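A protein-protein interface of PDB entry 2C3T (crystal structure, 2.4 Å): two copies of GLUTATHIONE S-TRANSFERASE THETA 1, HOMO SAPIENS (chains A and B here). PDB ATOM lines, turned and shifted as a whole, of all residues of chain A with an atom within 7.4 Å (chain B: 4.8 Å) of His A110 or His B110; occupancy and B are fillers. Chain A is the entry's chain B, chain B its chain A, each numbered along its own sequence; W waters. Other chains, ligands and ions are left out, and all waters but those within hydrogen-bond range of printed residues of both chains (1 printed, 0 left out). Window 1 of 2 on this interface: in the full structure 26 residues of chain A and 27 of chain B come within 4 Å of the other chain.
NH1 of Arg A247 sits at hydrogen-bond distance from O of Thr B111 (3.0 Å).
The backbone carbonyl oxygen of His B110 is in hydrogen-bond range of the guanidinium group of Arg B114, 2.9 Å away. The backbone carbonyl oxygen (O) of Leu A106 lies within hydrogen-bond range of a ring nitrogen (ND1) of His A110. The backbone carbonyl oxygen (O) of His A110 sits at hydrogen-bond distance from the guanidinium group (NE) of Arg A114 (2.7 Å). The backbone carbonyl oxygen (O) of Trp B108 sits at hydrogen-bond distance from the side-chain hydroxyl (OG1) of Thr B112, 2.9 Å away. The backbone carbonyl oxygen (O) of Ala A107 is in hydrogen-bond range of a ring nitrogen (ND1) of His A110 (3.4 Å). The chain-end carboxylate (O) of Arg A247 lies within salt-bridge range of the guanidinium group (NE) of Arg A115.
Among the printed residues, pairs that only touch across the chains: Glu A73 with Ala B107, Glu A73 with Trp B108, Ala A107 with His B110, His A110 with Ala B107, His A110 with His B110, His A110 with Thr B111, Thr A111 with His B110, Thr A111 with Arg B114, Arg A114 with Thr B111 and Arg A247 with Arg B115.
His A110 touches three residues of chain B. Of the printed residues of chain B, Arg A114 touches Thr B111. Arg A115 touches none of the printed residues of chain B. Glu A180 touches none of the printed residues of chain B. His B110 touches just these residues of chain A: Ala A107, His A110 and Thr A111. Printed residues of chain A within 4 Å of Arg B114: Thr A111 (3.5 Å). The nearest printed residue of chain B that does not touch His A110 is Leu B106 (5.2 Å).
Hydrophobic or aromatic side chains of chain B within 4 Å of the printed part of chain A: Ala B107, Trp B108 and His B110.
Ala A107 touches His B110, and with the chains exchanged His A110 touches Ala B107. His B110 touches its own counterpart, His A110. His A110 touches Thr B111, and with the chains exchanged Thr A111 touches His B110. Thr A111 touches Arg B114, and with the chains exchanged Arg A114 touches Thr B111.
Water W1 lies within hydrogen-bond range of O of Ala A107 (2.6 Å), OG1 of Thr A111 (3.1 Å) and ND1 of His B110 (3.4 Å).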
ATOM      1  N   GLU A  73      37.382  11.656  10.172  1.00  0.00           N
ATOM      2  CA  GLU A  73      36.540  10.476   9.802  1.00  0.00           C
ATOM      3  C   GLU A  73      37.258   9.155  10.143  1.00  0.00           C
ATOM      4  O   GLU A  73      38.244   8.795   9.489  1.00  0.00           O
ATOM      5  CB  GLU A  73      36.098  10.524   8.325  1.00  0.00           C
ATOM      6  CG  GLU A  73      35.366  11.838   7.940  1.00  0.00           C
ATOM      7  CD  GLU A  73      34.143  12.130   8.827  1.00  0.00           C
ATOM      8  OE1 GLU A  73      33.528  11.168   9.375  1.00  0.00           O
ATOM      9  OE2 GLU A  73      33.759  13.311   8.918  1.00  0.00           O
ATOM     10  N   SER A  74      36.753   8.422  11.161  1.00  0.00           N
ATOM     11  CA  SER A  74      37.422   7.137  11.583  1.00  0.00           C
ATOM     12  C   SER A  74      37.502   6.137  10.457  1.00  0.00           C
ATOM     13  O   SER A  74      38.458   5.354  10.386  1.00  0.00           O
ATOM     14  CB  SER A  74      36.730   6.489  12.818  1.00  0.00           C
ATOM     15  OG  SER A  74      35.419   6.045  12.526  1.00  0.00           O
ATOM     16  N   VAL A  75      36.515   6.157   9.558  1.00  0.00           N
ATOM     17  CA  VAL A  75      36.527   5.217   8.411  1.00  0.00           C
ATOM     18  C   VAL A  75      37.733   5.497   7.499  1.00  0.00           C
ATOM     19  O   VAL A  75      38.401   4.563   7.034  1.00  0.00           O
ATOM     20  CB  VAL A  75      35.202   5.244   7.605  1.00  0.00           C
ATOM     21  CG1 VAL A  75      35.327   4.434   6.346  1.00  0.00           C
ATOM     22  CG2 VAL A  75      34.032   4.735   8.469  1.00  0.00           C
ATOM     23  N   ALA A  76      38.078   6.780   7.354  1.00  0.00           N
ATOM     24  CA  ALA A  76      39.203   7.185   6.529  1.00  0.00           C
ATOM     25  C   ALA A  76      40.490   6.885   7.263  1.00  0.00           C
ATOM     26  O   ALA A  76      41.478   6.467   6.655  1.00  0.00           O
ATOM     27  CB  ALA A  76      39.113   8.638   6.214  1.00  0.00           C
ATOM     28  N   ASP A 103      33.188  -2.383   3.179  1.00  0.00           N
ATOM     29  CA  ASP A 103      32.756  -1.037   2.756  1.00  0.00           C
ATOM     30  C   ASP A 103      31.259  -0.864   2.903  1.00  0.00           C
ATOM     31  O   ASP A 103      30.793   0.194   3.314  1.00  0.00           O
ATOM     32  CB  ASP A 103      33.146  -0.757   1.309  1.00  0.00           C
ATOM     33  CG  ASP A 103      34.648  -0.742   1.091  1.00  0.00           C
ATOM     34  OD1 ASP A 103      35.411  -0.496   2.065  1.00  0.00           O
ATOM     35  OD2 ASP A 103      35.061  -0.879  -0.081  1.00  0.00           O
ATOM     36  N   TYR A 105      29.189  -2.265   5.061  1.00  0.00           N
ATOM     37  CA  TYR A 105      28.854  -2.026   6.446  1.00  0.00           C
ATOM     38  C   TYR A 105      29.294  -0.620   6.891  1.00  0.00           C
ATOM     39  O   TYR A 105      28.496   0.141   7.472  1.00  0.00           O
ATOM     40  CB  TYR A 105      29.476  -3.094   7.401  1.00  0.00           C
ATOM     41  CG  TYR A 105      29.155  -2.770   8.833  1.00  0.00           C
ATOM     42  CD1 TYR A 105      27.905  -3.130   9.382  1.00  0.00           C
ATOM     43  CD2 TYR A 105      29.978  -1.929   9.574  1.00  0.00           C
ATOM     44  CE1 TYR A 105      27.516  -2.690  10.606  1.00  0.00           C
ATOM     45  CE2 TYR A 105      29.601  -1.496  10.825  1.00  0.00           C
ATOM     46  CZ  TYR A 105      28.360  -1.891  11.342  1.00  0.00           C
ATOM     47  OH  TYR A 105      27.977  -1.487  12.586  1.00  0.00           O
ATOM     48  N   LEU A 106      30.552  -0.270   6.590  1.00  0.00           N
ATOM     49  CA  LEU A 106      31.120   1.042   6.989  1.00  0.00           C
ATOM     50  C   LEU A 106      30.324   2.218   6.449  1.00  0.00           C
ATOM     51  O   LEU A 106      30.243   3.247   7.086  1.00  0.00           O
ATOM     52  CB  LEU A 106      32.608   1.154   6.555  1.00  0.00           C
ATOM     53  CG  LEU A 106      33.600   0.180   7.206  1.00  0.00           C
ATOM     54  CD1 LEU A 106      35.009   0.488   6.727  1.00  0.00           C
ATOM     55  CD2 LEU A 106      33.535   0.243   8.710  1.00  0.00           C
ATOM     56  N   ALA A 107      29.741   2.053   5.267  1.00  0.00           N
ATOM     57  CA  ALA A 107      28.948   3.092   4.676  1.00  0.00           C
ATOM     58  C   ALA A 107      27.555   3.118   5.304  1.00  0.00           C
ATOM     59  O   ALA A 107      26.999   4.186   5.572  1.00  0.00           O
ATOM     60  CB  ALA A 107      28.855   2.908   3.153  1.00  0.00           C
ATOM     61  N   TRP A 108      27.058   1.928   5.641  1.00  0.00           N
ATOM     62  CA  TRP A 108      25.733   1.760   6.238  1.00  0.00           C
ATOM     63  C   TRP A 108      25.598   2.290   7.670  1.00  0.00           C
ATOM     64  O   TRP A 108      24.644   2.998   7.977  1.00  0.00           O
ATOM     65  CB  TRP A 108      25.333   0.255   6.224  1.00  0.00           C
ATOM     66  CG  TRP A 108      24.018   0.009   6.850  1.00  0.00           C
ATOM     67  CD1 TRP A 108      22.780   0.152   6.256  1.00  0.00           C
ATOM     68  CD2 TRP A 108      23.771  -0.422   8.197  1.00  0.00           C
ATOM     69  NE1 TRP A 108      21.794  -0.129   7.162  1.00  0.00           N
ATOM     70  CE2 TRP A 108      22.366  -0.486   8.361  1.00  0.00           C
ATOM     71  CE3 TRP A 108      24.602  -0.731   9.298  1.00  0.00           C
ATOM     72  CZ2 TRP A 108      21.766  -0.861   9.575  1.00  0.00           C
ATOM     73  CZ3 TRP A 108      24.005  -1.108  10.500  1.00  0.00           C
ATOM     74  CH2 TRP A 108      22.599  -1.170  10.627  1.00  0.00           C
ATOM     75  N   GLN A 109      26.560   1.963   8.527  1.00  0.00           N
ATOM     76  CA  GLN A 109      26.500   2.380   9.972  1.00  0.00           C
ATOM     77  C   GLN A 109      26.440   3.924  10.269  1.00  0.00           C
ATOM     78  O   GLN A 109      25.904   4.304  11.294  1.00  0.00           O
ATOM     79  CB  GLN A 109      27.679   1.707  10.774  1.00  0.00           C
ATOM     80  CG  GLN A 109      29.105   2.010  10.282  1.00  0.00           C
ATOM     81  CD  GLN A 109      29.593   3.411  10.608  1.00  0.00           C
ATOM     82  OE1 GLN A 109      29.207   3.996  11.621  1.00  0.00           O
ATOM     83  NE2 GLN A 109      30.577   3.871   9.856  1.00  0.00           N
ATOM     84  N   HIS A 110      26.929   4.778   9.357  1.00  0.00           N
ATOM     85  CA  HIS A 110      26.919   6.286   9.609  1.00  0.00           C
ATOM     86  C   HIS A 110      25.582   6.866  10.059  1.00  0.00           C
ATOM     87  O   HIS A 110      25.506   7.549  11.090  1.00  0.00           O
ATOM     88  CB  HIS A 110      27.410   7.105   8.372  1.00  0.00           C
ATOM     89  CG  HIS A 110      28.871   6.972   8.084  1.00  0.00           C
ATOM     90  ND1 HIS A 110      29.367   6.182   7.064  1.00  0.00           N
ATOM     91  CD2 HIS A 110      29.948   7.522   8.691  1.00  0.00           C
ATOM     92  CE1 HIS A 110      30.685   6.283   7.035  1.00  0.00           C
ATOM     93  NE2 HIS A 110      31.064   7.072   8.024  1.00  0.00           N
ATOM     94  N   THR A 111      24.531   6.569   9.286  1.00  0.00           N
ATOM     95  CA  THR A 111      23.185   7.096   9.543  1.00  0.00           C
ATOM     96  C   THR A 111      22.239   6.169  10.310  1.00  0.00           C
ATOM     97  O   THR A 111      21.150   6.586  10.706  1.00  0.00           O
ATOM     98  CB  THR A 111      22.497   7.486   8.179  1.00  0.00           C
ATOM     99  OG1 THR A 111      22.381   6.324   7.335  1.00  0.00           O
ATOM    100  CG2 THR A 111      23.293   8.514   7.473  1.00  0.00           C
ATOM    101  N   THR A 112      22.672   4.954  10.588  1.00  0.00           N
ATOM    102  CA  THR A 112      21.800   3.992  11.297  1.00  0.00           C
ATOM    103  C   THR A 112      22.278   3.623  12.712  1.00  0.00           C
ATOM    104  O   THR A 112      21.933   4.303  13.695  1.00  0.00           O
ATOM    105  CB  THR A 112      21.655   2.700  10.472  1.00  0.00           C
ATOM    106  OG1 THR A 112      22.941   2.156  10.234  1.00  0.00           O
ATOM    107  CG2 THR A 112      20.991   2.983   9.129  1.00  0.00           C
ATOM    108  N   LEU A 113      23.086   2.561  12.804  1.00  0.00           N
ATOM    109  CA  LEU A 113      23.605   2.054  14.096  1.00  0.00           C
ATOM    110  C   LEU A 113      24.438   3.113  14.894  1.00  0.00           C
ATOM    111  O   LEU A 113      24.388   3.134  16.131  1.00  0.00           O
ATOM    112  CB  LEU A 113      24.425   0.781  13.883  1.00  0.00           C
ATOM    113  CG  LEU A 113      24.759  -0.006  15.136  1.00  0.00           C
ATOM    114  CD1 LEU A 113      23.463  -0.541  15.765  1.00  0.00           C
ATOM    115  CD2 LEU A 113      25.660  -1.121  14.812  1.00  0.00           C
ATOM    116  N   ARG A 114      25.237   3.929  14.197  1.00  0.00           N
ATOM    117  CA  ARG A 114      26.002   4.945  14.877  1.00  0.00           C
ATOM    118  C   ARG A 114      25.028   5.961  15.457  1.00  0.00           C
ATOM    119  O   ARG A 114      25.162   6.365  16.587  1.00  0.00           O
ATOM    120  CB  ARG A 114      26.946   5.646  13.949  1.00  0.00           C
ATOM    121  CG  ARG A 114      27.841   6.687  14.649  1.00  0.00           C
ATOM    122  CD  ARG A 114      28.398   7.683  13.640  1.00  0.00           C
ATOM    123  NE  ARG A 114      27.268   8.328  12.959  1.00  0.00           N
ATOM    124  CZ  ARG A 114      26.629   9.416  13.405  1.00  0.00           C
ATOM    125  NH1 ARG A 114      27.039  10.036  14.491  1.00  0.00           N
ATOM    126  NH2 ARG A 114      25.597   9.893  12.739  1.00  0.00           N
ATOM    127  N   ARG A 115      24.045   6.365  14.655  1.00  0.00           N
ATOM    128  CA  ARG A 115      23.033   7.333  15.076  1.00  0.00           C
ATOM    129  C   ARG A 115      22.206   6.842  16.295  1.00  0.00           C
ATOM    130  O   ARG A 115      21.962   7.589  17.220  1.00  0.00           O
ATOM    131  CB  ARG A 115      22.104   7.659  13.916  1.00  0.00           C
ATOM    132  CG  ARG A 115      21.011   8.639  14.251  1.00  0.00           C
ATOM    133  CD  ARG A 115      20.078   8.831  13.090  1.00  0.00           C
ATOM    134  NE  ARG A 115      19.067   9.842  13.391  1.00  0.00           N
ATOM    135  CZ  ARG A 115      17.893   9.591  13.969  1.00  0.00           C
ATOM    136  NH1 ARG A 115      17.555   8.354  14.286  1.00  0.00           N
ATOM    137  NH2 ARG A 115      17.050  10.588  14.207  1.00  0.00           N
ATOM    138  N   SER A 116      21.796   5.569  16.253  1.00  0.00           N
ATOM    139  CA  SER A 116      21.003   4.943  17.317  1.00  0.00           C
ATOM    140  C   SER A 116      21.719   4.895  18.618  1.00  0.00           C
ATOM    141  O   SER A 116      21.193   5.325  19.637  1.00  0.00           O
ATOM    142  CB  SER A 116      20.645   3.500  16.922  1.00  0.00           C
ATOM    143  OG  SER A 116      19.897   3.467  15.753  1.00  0.00           O
ATOM    144  N   VAL A 176      34.185  -1.504  14.184  1.00  0.00           N
ATOM    145  CA  VAL A 176      33.339  -0.297  14.252  1.00  0.00           C
ATOM    146  C   VAL A 176      31.978  -0.570  14.919  1.00  0.00           C
ATOM    147  O   VAL A 176      31.479   0.248  15.692  1.00  0.00           O
ATOM    148  CB  VAL A 176      33.114   0.330  12.847  1.00  0.00           C
ATOM    149  CG1 VAL A 176      32.075   1.448  12.896  1.00  0.00           C
ATOM    150  CG2 VAL A 176      34.430   0.842  12.270  1.00  0.00           C
ATOM    151  N   GLU A 180      30.368   0.717  18.724  1.00  0.00           N
ATOM    152  CA  GLU A 180      29.101   1.446  18.605  1.00  0.00           C
ATOM    153  C   GLU A 180      28.147   0.903  19.599  1.00  0.00           C
ATOM    154  O   GLU A 180      27.568   1.649  20.372  1.00  0.00           O
ATOM    155  CB  GLU A 180      28.510   1.357  17.166  1.00  0.00           C
ATOM    156  CG  GLU A 180      29.268   2.170  16.175  1.00  0.00           C
ATOM    157  CD  GLU A 180      28.790   2.024  14.756  1.00  0.00           C
ATOM    158  OE1 GLU A 180      28.356   0.908  14.357  1.00  0.00           O
ATOM    159  OE2 GLU A 180      29.029   2.965  13.985  1.00  0.00           O
ATOM    160  N   ARG A 247      21.389  13.927  15.470  1.00  0.00           N
ATOM    161  CA  ARG A 247      20.129  13.884  14.667  1.00  0.00           C
ATOM    162  C   ARG A 247      20.258  12.971  13.422  1.00  0.00           C
ATOM    163  O   ARG A 247      19.250  12.602  12.810  1.00  0.00           O
ATOM    164  CB  ARG A 247      19.610  15.316  14.269  1.00  0.00           C
ATOM    165  CG  ARG A 247      20.326  16.038  13.088  1.00  0.00           C
ATOM    166  CD  ARG A 247      21.759  16.308  13.285  1.00  0.00           C
ATOM    167  NE  ARG A 247      22.314  17.044  12.135  1.00  0.00           N
ATOM    168  CZ  ARG A 247      22.860  16.473  11.054  1.00  0.00           C
ATOM    169  NH1 ARG A 247      22.971  15.141  10.971  1.00  0.00           N
ATOM    170  NH2 ARG A 247      23.325  17.237  10.062  1.00  0.00           N
ATOM    171  OXT ARG A 247      21.357  12.546  13.042  1.00  0.00           O
ATOM    172  N   VAL B  75      28.591   4.137  -1.794  1.00  0.00           N
ATOM    173  CA  VAL B  75      30.058   4.224  -1.577  1.00  0.00           C
ATOM    174  C   VAL B  75      30.740   2.872  -1.832  1.00  0.00           C
ATOM    175  O   VAL B  75      31.745   2.799  -2.518  1.00  0.00           O
ATOM    176  CB  VAL B  75      30.409   4.779  -0.155  1.00  0.00           C
ATOM    177  CG1 VAL B  75      31.926   4.745   0.102  1.00  0.00           C
ATOM    178  CG2 VAL B  75      29.873   6.170   0.003  1.00  0.00           C
ATOM    179  N   LEU B 106      33.897  10.839   1.423  1.00  0.00           N
ATOM    180  CA  LEU B 106      32.803   9.816   1.275  1.00  0.00           C
ATOM    181  C   LEU B 106      32.191   9.421   2.581  1.00  0.00           C
ATOM    182  O   LEU B 106      31.023   9.143   2.646  1.00  0.00           O
ATOM    183  CB  LEU B 106      33.320   8.546   0.491  1.00  0.00           C
ATOM    184  CG  LEU B 106      33.706   8.744  -1.002  1.00  0.00           C
ATOM    185  CD1 LEU B 106      34.171   7.454  -1.598  1.00  0.00           C
ATOM    186  CD2 LEU B 106      32.552   9.297  -1.819  1.00  0.00           C
ATOM    187  N   ALA B 107      32.988   9.474   3.646  1.00  0.00           N
ATOM    188  CA  ALA B 107      32.527   9.143   4.978  1.00  0.00           C
ATOM    189  C   ALA B 107      31.815  10.331   5.610  1.00  0.00           C
ATOM    190  O   ALA B 107      30.778  10.174   6.280  1.00  0.00           O
ATOM    191  CB  ALA B 107      33.693   8.701   5.850  1.00  0.00           C
ATOM    192  N   TRP B 108      32.373  11.520   5.407  1.00  0.00           N
ATOM    193  CA  TRP B 108      31.802  12.766   5.959  1.00  0.00           C
ATOM    194  C   TRP B 108      30.413  13.112   5.425  1.00  0.00           C
ATOM    195  O   TRP B 108      29.509  13.409   6.191  1.00  0.00           O
ATOM    196  CB  TRP B 108      32.744  13.943   5.675  1.00  0.00           C
ATOM    197  CG  TRP B 108      32.179  15.323   6.114  1.00  0.00           C
ATOM    198  CD1 TRP B 108      32.307  15.912   7.338  1.00  0.00           C
ATOM    199  CD2 TRP B 108      31.460  16.280   5.283  1.00  0.00           C
ATOM    200  NE1 TRP B 108      31.694  17.156   7.335  1.00  0.00           N
ATOM    201  CE2 TRP B 108      31.171  17.399   6.091  1.00  0.00           C
ATOM    202  CE3 TRP B 108      31.045  16.289   3.944  1.00  0.00           C
ATOM    203  CZ2 TRP B 108      30.469  18.516   5.605  1.00  0.00           C
ATOM    204  CZ3 TRP B 108      30.350  17.383   3.470  1.00  0.00           C
ATOM    205  CH2 TRP B 108      30.071  18.488   4.300  1.00  0.00           C
ATOM    206  N   GLN B 109      30.250  13.018   4.107  1.00  0.00           N
ATOM    207  CA  GLN B 109      28.967  13.378   3.425  1.00  0.00           C
ATOM    208  C   GLN B 109      27.641  12.640   3.906  1.00  0.00           C
ATOM    209  O   GLN B 109      26.579  13.244   3.891  1.00  0.00           O
ATOM    210  CB  GLN B 109      29.151  13.253   1.846  1.00  0.00           C
ATOM    211  CG  GLN B 109      29.528  11.845   1.291  1.00  0.00           C
ATOM    212  CD  GLN B 109      28.393  10.869   1.306  1.00  0.00           C
ATOM    213  OE1 GLN B 109      27.249  11.243   1.465  1.00  0.00           O
ATOM    214  NE2 GLN B 109      28.691   9.630   1.024  1.00  0.00           N
ATOM    215  N   HIS B 110      27.755  11.409   4.402  1.00  0.00           N
ATOM    216  CA  HIS B 110      26.550  10.624   4.853  1.00  0.00           C
ATOM    217  C   HIS B 110      25.599  11.357   5.817  1.00  0.00           C
ATOM    218  O   HIS B 110      24.388  11.407   5.592  1.00  0.00           O
ATOM    219  CB  HIS B 110      26.971   9.291   5.509  1.00  0.00           C
ATOM    220  CG  HIS B 110      27.720   8.376   4.605  1.00  0.00           C
ATOM    221  ND1 HIS B 110      27.089   7.480   3.769  1.00  0.00           N
ATOM    222  CD2 HIS B 110      29.042   8.106   4.512  1.00  0.00           C
ATOM    223  CE1 HIS B 110      27.999   6.759   3.132  1.00  0.00           C
ATOM    224  NE2 HIS B 110      29.191   7.114   3.572  1.00  0.00           N
ATOM    225  N   THR B 111      26.163  11.881   6.896  1.00  0.00           N
ATOM    226  CA  THR B 111      25.400  12.579   7.943  1.00  0.00           C
ATOM    227  C   THR B 111      25.360  14.082   7.827  1.00  0.00           C
ATOM    228  O   THR B 111      24.878  14.760   8.732  1.00  0.00           O
ATOM    229  CB  THR B 111      26.003  12.250   9.343  1.00  0.00           C
ATOM    230  OG1 THR B 111      27.384  12.620   9.351  1.00  0.00           O
ATOM    231  CG2 THR B 111      25.904  10.799   9.629  1.00  0.00           C
ATOM    232  N   THR B 112      25.860  14.614   6.725  1.00  0.00           N
ATOM    233  CA  THR B 112      25.898  16.065   6.541  1.00  0.00           C
ATOM    234  C   THR B 112      25.278  16.554   5.196  1.00  0.00           C
ATOM    235  O   THR B 112      24.070  16.828   5.124  1.00  0.00           O
ATOM    236  CB  THR B 112      27.359  16.597   6.667  1.00  0.00           C
ATOM    237  OG1 THR B 112      28.182  15.957   5.744  1.00  0.00           O
ATOM    238  CG2 THR B 112      27.952  16.402   8.147  1.00  0.00           C
ATOM    239  N   ARG B 114      24.605  14.908   2.439  1.00  0.00           N
ATOM    240  CA  ARG B 114      23.608  14.004   1.907  1.00  0.00           C
ATOM    241  C   ARG B 114      22.279  14.325   2.538  1.00  0.00           C
ATOM    242  O   ARG B 114      21.274  14.438   1.855  1.00  0.00           O
ATOM    243  CB  ARG B 114      23.940  12.578   2.214  1.00  0.00           C
ATOM    244  CG  ARG B 114      22.971  11.556   1.566  1.00  0.00           C
ATOM    245  CD  ARG B 114      23.123  10.212   2.198  1.00  0.00           C
ATOM    246  NE  ARG B 114      22.682  10.275   3.592  1.00  0.00           N
ATOM    247  CZ  ARG B 114      21.443   9.984   4.012  1.00  0.00           C
ATOM    248  NH1 ARG B 114      20.550   9.469   3.166  1.00  0.00           N
ATOM    249  NH2 ARG B 114      21.132  10.107   5.301  1.00  0.00           N
ATOM    250  N   ARG B 115      22.297  14.491   3.865  1.00  0.00           N
ATOM    251  CA  ARG B 115      21.095  14.798   4.650  1.00  0.00           C
ATOM    252  C   ARG B 115      20.511  16.211   4.352  1.00  0.00           C
ATOM    253  O   ARG B 115      19.293  16.368   4.235  1.00  0.00           O
ATOM    254  CB  ARG B 115      21.396  14.660   6.137  1.00  0.00           C
ATOM    255  CG  ARG B 115      20.220  14.949   7.036  1.00  0.00           C
ATOM    256  CD  ARG B 115      20.621  14.891   8.482  1.00  0.00           C
ATOM    257  NE  ARG B 115      19.508  15.214   9.364  1.00  0.00           N
ATOM    258  CZ  ARG B 115      19.185  16.454   9.756  1.00  0.00           C
ATOM    259  NH1 ARG B 115      19.881  17.511   9.316  1.00  0.00           N
ATOM    260  NH2 ARG B 115      18.153  16.641  10.562  1.00  0.00           N
HETATM  261  O   HOH W   1      25.040   5.882   5.907  1.00  0.00           O
